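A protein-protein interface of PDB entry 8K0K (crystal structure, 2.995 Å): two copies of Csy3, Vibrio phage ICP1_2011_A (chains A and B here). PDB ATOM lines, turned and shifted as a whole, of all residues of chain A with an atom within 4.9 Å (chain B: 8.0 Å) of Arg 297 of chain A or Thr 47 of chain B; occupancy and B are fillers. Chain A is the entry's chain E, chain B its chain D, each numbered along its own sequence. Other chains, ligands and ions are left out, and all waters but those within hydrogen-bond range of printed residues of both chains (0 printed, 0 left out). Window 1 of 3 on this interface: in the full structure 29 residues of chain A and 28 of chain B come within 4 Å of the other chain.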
ATOM      1  N   ARG A  14     -21.841  20.093 -18.579  1.00  0.00           N
ATOM      2  CA  ARG A  14     -21.896  18.982 -17.639  1.00  0.00           C
ATOM      3  C   ARG A  14     -21.840  19.485 -16.201  1.00  0.00           C
ATOM      4  O   ARG A  14     -21.318  20.567 -15.914  1.00  0.00           O
ATOM      5  CB  ARG A  14     -20.749  18.002 -17.886  1.00  0.00           C
ATOM      6  CG  ARG A  14     -19.471  18.372 -17.161  1.00  0.00           C
ATOM      7  CD  ARG A  14     -18.425  17.286 -17.269  1.00  0.00           C
ATOM      8  NE  ARG A  14     -17.966  17.111 -18.642  1.00  0.00           N
ATOM      9  CZ  ARG A  14     -17.067  17.890 -19.234  1.00  0.00           C
ATOM     10  NH1 ARG A  14     -16.531  18.911 -18.584  1.00  0.00           N
ATOM     11  NH2 ARG A  14     -16.710  17.649 -20.483  1.00  0.00           N
ATOM     12  N   ARG A 234     -22.780   7.970 -13.864  1.00  0.00           N
ATOM     13  CA  ARG A 234     -24.143   8.220 -14.315  1.00  0.00           C
ATOM     14  C   ARG A 234     -24.916   6.942 -14.650  1.00  0.00           C
ATOM     15  O   ARG A 234     -26.057   7.032 -15.116  1.00  0.00           O
ATOM     16  CB  ARG A 234     -24.128   9.183 -15.511  1.00  0.00           C
ATOM     17  CG  ARG A 234     -24.262   8.556 -16.895  1.00  0.00           C
ATOM     18  CD  ARG A 234     -24.261   9.634 -17.972  1.00  0.00           C
ATOM     19  NE  ARG A 234     -22.902  10.078 -18.248  1.00  0.00           N
ATOM     20  CZ  ARG A 234     -22.263   9.848 -19.389  1.00  0.00           C
ATOM     21  NH1 ARG A 234     -21.015  10.273 -19.545  1.00  0.00           N
ATOM     22  NH2 ARG A 234     -22.879   9.207 -20.375  1.00  0.00           N
ATOM     23  N   VAL A 249     -26.830   7.030 -18.382  1.00  0.00           N
ATOM     24  CA  VAL A 249     -27.809   7.976 -18.901  1.00  0.00           C
ATOM     25  C   VAL A 249     -27.332   8.484 -20.255  1.00  0.00           C
ATOM     26  O   VAL A 249     -26.279   9.125 -20.360  1.00  0.00           O
ATOM     27  CB  VAL A 249     -28.035   9.126 -17.913  1.00  0.00           C
ATOM     28  CG1 VAL A 249     -28.917  10.196 -18.529  1.00  0.00           C
ATOM     29  CG2 VAL A 249     -28.670   8.598 -16.644  1.00  0.00           C
ATOM     30  N   GLU A 250     -28.094   8.181 -21.302  1.00  0.00           N
ATOM     31  CA  GLU A 250     -27.840   8.664 -22.652  1.00  0.00           C
ATOM     32  C   GLU A 250     -29.164   9.087 -23.266  1.00  0.00           C
ATOM     33  O   GLU A 250     -30.202   8.468 -22.995  1.00  0.00           O
ATOM     34  CB  GLU A 250     -27.189   7.595 -23.544  1.00  0.00           C
ATOM     35  CG  GLU A 250     -25.983   6.911 -22.937  1.00  0.00           C
ATOM     36  CD  GLU A 250     -24.751   7.791 -22.929  1.00  0.00           C
ATOM     37  OE1 GLU A 250     -24.823   8.916 -23.467  1.00  0.00           O
ATOM     38  OE2 GLU A 250     -23.706   7.355 -22.392  1.00  0.00           O
ATOM     39  N   PRO A 251     -29.163  10.139 -24.092  1.00  0.00           N
ATOM     40  CA  PRO A 251     -30.418  10.595 -24.712  1.00  0.00           C
ATOM     41  C   PRO A 251     -31.216   9.496 -25.393  1.00  0.00           C
ATOM     42  O   PRO A 251     -32.451   9.559 -25.396  1.00  0.00           O
ATOM     43  CB  PRO A 251     -29.954  11.655 -25.723  1.00  0.00           C
ATOM     44  CG  PRO A 251     -28.499  11.899 -25.449  1.00  0.00           C
ATOM     45  CD  PRO A 251     -28.083  11.122 -24.243  1.00  0.00           C
ATOM     46  N   SER A 254     -28.248   4.509 -25.179  1.00  0.00           N
ATOM     47  CA  SER A 254     -27.373   3.713 -26.025  1.00  0.00           C
ATOM     48  C   SER A 254     -26.289   3.037 -25.200  1.00  0.00           C
ATOM     49  O   SER A 254     -25.637   3.680 -24.371  1.00  0.00           O
ATOM     50  CB  SER A 254     -26.725   4.601 -27.079  1.00  0.00           C
ATOM     51  OG  SER A 254     -27.498   5.765 -27.309  1.00  0.00           O
ATOM     52  N   VAL A 256     -23.207   1.233 -26.749  1.00  0.00           N
ATOM     53  CA  VAL A 256     -22.662   0.905 -28.062  1.00  0.00           C
ATOM     54  C   VAL A 256     -21.846  -0.377 -28.018  1.00  0.00           C
ATOM     55  O   VAL A 256     -21.820  -1.133 -28.997  1.00  0.00           O
ATOM     56  CB  VAL A 256     -21.833   2.077 -28.617  1.00  0.00           C
ATOM     57  CG1 VAL A 256     -22.744   3.227 -28.986  1.00  0.00           C
ATOM     58  CG2 VAL A 256     -20.801   2.523 -27.602  1.00  0.00           C
ATOM     59  N   ALA A 293     -31.441  13.991 -15.591  1.00  0.00           N
ATOM     60  CA  ALA A 293     -30.148  13.322 -15.659  1.00  0.00           C
ATOM     61  C   ALA A 293     -29.443  13.635 -16.968  1.00  0.00           C
ATOM     62  O   ALA A 293     -28.215  13.752 -17.008  1.00  0.00           O
ATOM     63  CB  ALA A 293     -30.327  11.814 -15.489  1.00  0.00           C
ATOM     64  N   ASN A 294     -30.209  13.778 -18.052  1.00  0.00           N
ATOM     65  CA  ASN A 294     -29.607  14.201 -19.313  1.00  0.00           C
ATOM     66  C   ASN A 294     -29.162  15.657 -19.253  1.00  0.00           C
ATOM     67  O   ASN A 294     -28.101  16.007 -19.781  1.00  0.00           O
ATOM     68  CB  ASN A 294     -30.581  13.987 -20.467  1.00  0.00           C
ATOM     69  CG  ASN A 294     -30.557  12.571 -20.982  1.00  0.00           C
ATOM     70  OD1 ASN A 294     -29.651  12.185 -21.718  1.00  0.00           O
ATOM     71  ND2 ASN A 294     -31.545  11.780 -20.589  1.00  0.00           N
ATOM     72  N   LEU A 295     -29.962  16.524 -18.628  1.00  0.00           N
ATOM     73  CA  LEU A 295     -29.535  17.913 -18.472  1.00  0.00           C
ATOM     74  C   LEU A 295     -28.286  18.016 -17.602  1.00  0.00           C
ATOM     75  O   LEU A 295     -27.527  18.986 -17.713  1.00  0.00           O
ATOM     76  CB  LEU A 295     -30.660  18.759 -17.880  1.00  0.00           C
ATOM     77  CG  LEU A 295     -31.897  18.978 -18.747  1.00  0.00           C
ATOM     78  CD1 LEU A 295     -32.786  20.046 -18.140  1.00  0.00           C
ATOM     79  CD2 LEU A 295     -31.493  19.359 -20.146  1.00  0.00           C
ATOM     80  N   ILE A 296     -28.075  17.040 -16.720  1.00  0.00           N
ATOM     81  CA  ILE A 296     -26.864  16.998 -15.908  1.00  0.00           C
ATOM     82  C   ILE A 296     -25.700  16.438 -16.719  1.00  0.00           C
ATOM     83  O   ILE A 296     -24.550  16.869 -16.566  1.00  0.00           O
ATOM     84  CB  ILE A 296     -27.124  16.179 -14.627  1.00  0.00           C
ATOM     85  CG1 ILE A 296     -28.092  16.918 -13.706  1.00  0.00           C
ATOM     86  CG2 ILE A 296     -25.835  15.888 -13.880  1.00  0.00           C
ATOM     87  CD1 ILE A 296     -28.383  16.176 -12.423  1.00  0.00           C
ATOM     88  N   ARG A 297     -25.985  15.476 -17.598  1.00  0.00           N
ATOM     89  CA  ARG A 297     -24.943  14.893 -18.434  1.00  0.00           C
ATOM     90  C   ARG A 297     -24.295  15.948 -19.315  1.00  0.00           C
ATOM     91  O   ARG A 297     -23.072  15.953 -19.493  1.00  0.00           O
ATOM     92  CB  ARG A 297     -25.526  13.777 -19.299  1.00  0.00           C
ATOM     93  CG  ARG A 297     -24.489  12.834 -19.865  1.00  0.00           C
ATOM     94  CD  ARG A 297     -25.002  12.086 -21.086  1.00  0.00           C
ATOM     95  NE  ARG A 297     -24.924  12.902 -22.291  1.00  0.00           N
ATOM     96  CZ  ARG A 297     -24.734  12.409 -23.509  1.00  0.00           C
ATOM     97  NH1 ARG A 297     -24.598  11.105 -23.674  1.00  0.00           N
ATOM     98  NH2 ARG A 297     -24.668  13.218 -24.559  1.00  0.00           N
ATOM     99  N   GLY A 298     -25.099  16.854 -19.860  1.00  0.00           N
ATOM    100  CA  GLY A 298     -24.632  17.815 -20.830  1.00  0.00           C
ATOM    101  C   GLY A 298     -24.804  17.313 -22.250  1.00  0.00           C
ATOM    102  O   GLY A 298     -25.172  16.166 -22.508  1.00  0.00           O
ATOM    103  N   GLY A 299     -24.532  18.204 -23.194  1.00  0.00           N
ATOM    104  CA  GLY A 299     -24.626  17.890 -24.601  1.00  0.00           C
ATOM    105  C   GLY A 299     -25.447  18.911 -25.353  1.00  0.00           C
ATOM    106  O   GLY A 299     -25.992  19.857 -24.788  1.00  0.00           O
ATOM    107  N   VAL B  44     -11.188   9.694 -26.949  1.00  0.00           N
ATOM    108  CA  VAL B  44     -12.508   9.930 -26.378  1.00  0.00           C
ATOM    109  C   VAL B  44     -13.517   9.147 -27.202  1.00  0.00           C
ATOM    110  O   VAL B  44     -13.643   9.372 -28.410  1.00  0.00           O
ATOM    111  CB  VAL B  44     -12.871  11.424 -26.354  1.00  0.00           C
ATOM    112  CG1 VAL B  44     -14.358  11.608 -26.105  1.00  0.00           C
ATOM    113  CG2 VAL B  44     -12.069  12.138 -25.287  1.00  0.00           C
ATOM    114  N   ALA B  45     -14.224   8.223 -26.561  1.00  0.00           N
ATOM    115  CA  ALA B  45     -15.222   7.397 -27.225  1.00  0.00           C
ATOM    116  C   ALA B  45     -16.604   7.786 -26.724  1.00  0.00           C
ATOM    117  O   ALA B  45     -16.826   7.883 -25.512  1.00  0.00           O
ATOM    118  CB  ALA B  45     -14.965   5.910 -26.977  1.00  0.00           C
ATOM    119  N   GLY B  46     -17.527   8.006 -27.653  1.00  0.00           N
ATOM    120  CA  GLY B  46     -18.862   8.413 -27.274  1.00  0.00           C
ATOM    121  C   GLY B  46     -19.965   7.789 -28.098  1.00  0.00           C
ATOM    122  O   GLY B  46     -19.718   6.929 -28.950  1.00  0.00           O
ATOM    123  N   THR B  47     -21.189   8.242 -27.853  1.00  0.00           N
ATOM    124  CA  THR B  47     -22.388   7.775 -28.530  1.00  0.00           C
ATOM    125  C   THR B  47     -22.821   8.762 -29.609  1.00  0.00           C
ATOM    126  O   THR B  47     -22.439   9.934 -29.610  1.00  0.00           O
ATOM    127  CB  THR B  47     -23.527   7.578 -27.528  1.00  0.00           C
ATOM    128  OG1 THR B  47     -23.581   8.700 -26.634  1.00  0.00           O
ATOM    129  CG2 THR B  47     -23.318   6.302 -26.728  1.00  0.00           C
ATOM    130  N   GLN B  48     -23.638   8.262 -30.538  1.00  0.00           N
ATOM    131  CA  GLN B  48     -24.207   9.085 -31.605  1.00  0.00           C
ATOM    132  C   GLN B  48     -25.568   9.585 -31.136  1.00  0.00           C
ATOM    133  O   GLN B  48     -26.622   9.033 -31.460  1.00  0.00           O
ATOM    134  CB  GLN B  48     -24.309   8.286 -32.897  1.00  0.00           C
ATOM    135  CG  GLN B  48     -22.997   7.691 -33.351  1.00  0.00           C
ATOM    136  CD  GLN B  48     -22.500   8.301 -34.634  1.00  0.00           C
ATOM    137  OE1 GLN B  48     -21.710   9.246 -34.620  1.00  0.00           O
ATOM    138  NE2 GLN B  48     -22.962   7.767 -35.760  1.00  0.00           N
ATOM    139  N   SER B  49     -25.534  10.661 -30.355  1.00  0.00           N
ATOM    140  CA  SER B  49     -26.730  11.130 -29.669  1.00  0.00           C
ATOM    141  C   SER B  49     -27.199  12.470 -30.218  1.00  0.00           C
ATOM    142  O   SER B  49     -27.311  13.449 -29.471  1.00  0.00           O
ATOM    143  CB  SER B  49     -26.455  11.237 -28.169  1.00  0.00           C
ATOM    144  OG  SER B  49     -25.829  10.063 -27.680  1.00  0.00           O
ATOM    145  N   VAL B  50     -27.472  12.528 -31.518  1.00  0.00           N
ATOM    146  CA  VAL B  50     -27.974  13.741 -32.152  1.00  0.00           C
ATOM    147  C   VAL B  50     -29.491  13.751 -32.059  1.00  0.00           C
ATOM    148  O   VAL B  50     -30.138  12.702 -31.971  1.00  0.00           O
ATOM    149  CB  VAL B  50     -27.504  13.848 -33.615  1.00  0.00           C
ATOM    150  CG1 VAL B  50     -25.998  14.009 -33.674  1.00  0.00           C
ATOM    151  CG2 VAL B  50     -27.950  12.625 -34.396  1.00  0.00           C
ATOM    152  N   ASP B  56     -28.951   5.811 -35.724  1.00  0.00           N
ATOM    153  CA  ASP B  56     -27.541   5.694 -35.387  1.00  0.00           C
ATOM    154  C   ASP B  56     -27.315   5.596 -33.886  1.00  0.00           C
ATOM    155  O   ASP B  56     -26.162   5.615 -33.441  1.00  0.00           O
ATOM    156  CB  ASP B  56     -26.773   6.882 -35.960  1.00  0.00           C
ATOM    157  CG  ASP B  56     -27.166   7.187 -37.387  1.00  0.00           C
ATOM    158  OD1 ASP B  56     -27.121   6.262 -38.228  1.00  0.00           O
ATOM    159  OD2 ASP B  56     -27.540   8.345 -37.663  1.00  0.00           O
ATOM    160  N   ALA B  57     -28.385   5.483 -33.101  1.00  0.00           N
ATOM    161  CA  ALA B  57     -28.267   5.446 -31.651  1.00  0.00           C
ATOM    162  C   ALA B  57     -27.582   4.187 -31.142  1.00  0.00           C
ATOM    163  O   ALA B  57     -27.211   4.145 -29.968  1.00  0.00           O
ATOM    164  CB  ALA B  57     -29.644   5.573 -31.004  1.00  0.00           C
ATOM    165  N   ASP B  58     -27.410   3.168 -31.974  1.00  0.00           N
ATOM    166  CA  ASP B  58     -26.661   1.984 -31.585  1.00  0.00           C
ATOM    167  C   ASP B  58     -25.200   2.046 -32.015  1.00  0.00           C
ATOM    168  O   ASP B  58     -24.435   1.127 -31.704  1.00  0.00           O
ATOM    169  CB  ASP B  58     -27.323   0.731 -32.162  1.00  0.00           C
ATOM    170  CG  ASP B  58     -27.525   0.819 -33.665  1.00  0.00           C
ATOM    171  OD1 ASP B  58     -27.648   1.947 -34.192  1.00  0.00           O
ATOM    172  OD2 ASP B  58     -27.564  -0.241 -34.324  1.00  0.00           O
ATOM    173  N   LYS B  59     -24.796   3.107 -32.710  1.00  0.00           N
ATOM    174  CA  LYS B  59     -23.442   3.255 -33.221  1.00  0.00           C
ATOM    175  C   LYS B  59     -22.628   4.170 -32.312  1.00  0.00           C
ATOM    176  O   LYS B  59     -23.154   5.113 -31.716  1.00  0.00           O
ATOM    177  CB  LYS B  59     -23.461   3.812 -34.648  1.00  0.00           C
ATOM    178  CG  LYS B  59     -24.289   2.974 -35.618  1.00  0.00           C
ATOM    179  CD  LYS B  59     -24.542   3.705 -36.931  1.00  0.00           C
ATOM    180  CE  LYS B  59     -25.598   2.983 -37.764  1.00  0.00           C
ATOM    181  NZ  LYS B  59     -26.012   3.763 -38.968  1.00  0.00           N
ATOM    182  N   GLY B  60     -21.336   3.869 -32.195  1.00  0.00           N
ATOM    183  CA  GLY B  60     -20.429   4.662 -31.398  1.00  0.00           C
ATOM    184  C   GLY B  60     -19.586   5.587 -32.254  1.00  0.00           C
ATOM    185  O   GLY B  60     -19.784   5.717 -33.463  1.00  0.00           O
ATOM    186  N   ASN B  61     -18.631   6.251 -31.603  1.00  0.00           N
ATOM    187  CA  ASN B  61     -17.675   7.050 -32.358  1.00  0.00           C
ATOM    188  C   ASN B  61     -16.421   7.297 -31.530  1.00  0.00           C
ATOM    189  O   ASN B  61     -16.504   7.623 -30.345  1.00  0.00           O
ATOM    190  CB  ASN B  61     -18.285   8.384 -32.808  1.00  0.00           C
ATOM    191  CG  ASN B  61     -18.715   9.250 -31.649  1.00  0.00           C
ATOM    192  OD1 ASN B  61     -17.892   9.906 -31.013  1.00  0.00           O
ATOM    193  ND2 ASN B  61     -20.013   9.271 -31.376  1.00  0.00           N
ATOM    194  N   ILE B  62     -15.262   7.149 -32.174  1.00  0.00           N
ATOM    195  CA  ILE B  62     -13.973   7.441 -31.559  1.00  0.00           C
ATOM    196  C   ILE B  62     -13.495   8.799 -32.037  1.00  0.00           C
ATOM    197  O   ILE B  62     -13.771   9.219 -33.164  1.00  0.00           O
ATOM    198  CB  ILE B  62     -12.918   6.355 -31.869  1.00  0.00           C
ATOM    199  CG1 ILE B  62     -13.156   5.734 -33.252  1.00  0.00           C
ATOM    200  CG2 ILE B  62     -12.903   5.304 -30.781  1.00  0.00           C
ATOM    201  CD1 ILE B  62     -12.619   6.552 -34.432  1.00  0.00           C
ATOM    202  N   GLN B  63     -12.775   9.496 -31.166  1.00  0.00           N
ATOM    203  CA  GLN B  63     -12.102  10.737 -31.514  1.00  0.00           C
ATOM    204  C   GLN B  63     -10.815  10.810 -30.713  1.00  0.00           C
ATOM    205  O   GLN B  63     -10.620  10.069 -29.748  1.00  0.00           O
ATOM    206  CB  GLN B  63     -12.955  11.967 -31.200  1.00  0.00           C
ATOM    207  CG  GLN B  63     -14.349  11.985 -31.773  1.00  0.00           C
ATOM    208  CD  GLN B  63     -15.359  12.480 -30.757  1.00  0.00           C
ATOM    209  OE1 GLN B  63     -16.016  11.682 -30.092  1.00  0.00           O
ATOM    210  NE2 GLN B  63     -15.474  13.802 -30.618  1.00  0.00           N
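The side-chain hydroxyl (OG1) of Thr 47 of chain B sits at hydrogen-bond distance from the side-chain hydroxyl (OG) of Ser 49 of chain B (2.8 Å).
O of Thr 47 of chain B sits at hydrogen-bond distance from ND2 of Asn 61 of chain B, 3.1 Å away.
N of Gln 48 of chain B lies close to O of Lys 59 of chain B.
NZ of Lys 59 of chain B is in salt-bridge range of OD1 of Asp 56 of chain B, 2.8 Å away.
NH2 of Arg 234 of chain A is in salt-bridge range of OE2 of Glu 250 of chain A, 2.9 Å away.
No position is printed for both chains.
The side-chain carboxylate (OE1) of Glu 250 of chain A sits at hydrogen-bond distance from the side-chain hydroxyl (OG1) of Thr 47 of chain B, at 3.4 Å.
The side-chain hydroxyl of Ser 254 of chain A sits close to the backbone carbonyl oxygen of Ala 57 of chain B, 3.1 Å away.
CB of Ser 49 of chain B touches CG of Pro 251 of chain A, 3.5 Å away.
Thr 47 of chain B touches Ser 254 of chain A.
Val 256 of chain A touches Thr 47 of chain B.
Val 256 of chain A touches Asp 58 of chain B.
Lys 59 of chain B touches Val 256 of chain A (O to CG1, 3.3 Å).
N of Gly 60 of chain B touches CG1 of Val 256 of chain A (3.6 Å).
Arg 297 of chain A touches Thr 47 of chain B (NH1 to OG1, 3.9 Å).
Printed residues of chain B that touch a printed residue of chain A: Thr 47, Ser 49, Ala 57, Asp 58, Lys 59 and Gly 60.
Of the 14 printed residues of chain A, 5 touch a printed residue of chain B.
Hydrophobic or aromatic side chains of chain A within 4 Å of the printed part of chain B: Pro 251 and Val 256.
Among the printed residues, 9 pairs touch across the chains.
Arg 297 of chain A touches just one residue of chain B: Thr 47.
Of chain A, only Glu 250, Ser 254, Val 256 and Arg 297 come within 4 Å of Thr 47 of chain B.
No residue of chain B comes within 4 Å of Gly 298 of chain A.
Printed residues of chain A within 4 Å of Lys 59 of chain B: Val 256.
Of the printed residues of chain B, Ser 254 of chain A touches Thr 47 and Ala 57.
Of the printed residues of chain B, Glu 250 of chain A touches Thr 47 (3.4 Å).
Asn 294 of chain A touches none of the printed residues of chain B.
The nearest residue of chain B that does not touch Arg 297 of chain A is Ser 49 of chain B (4.3 Å).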
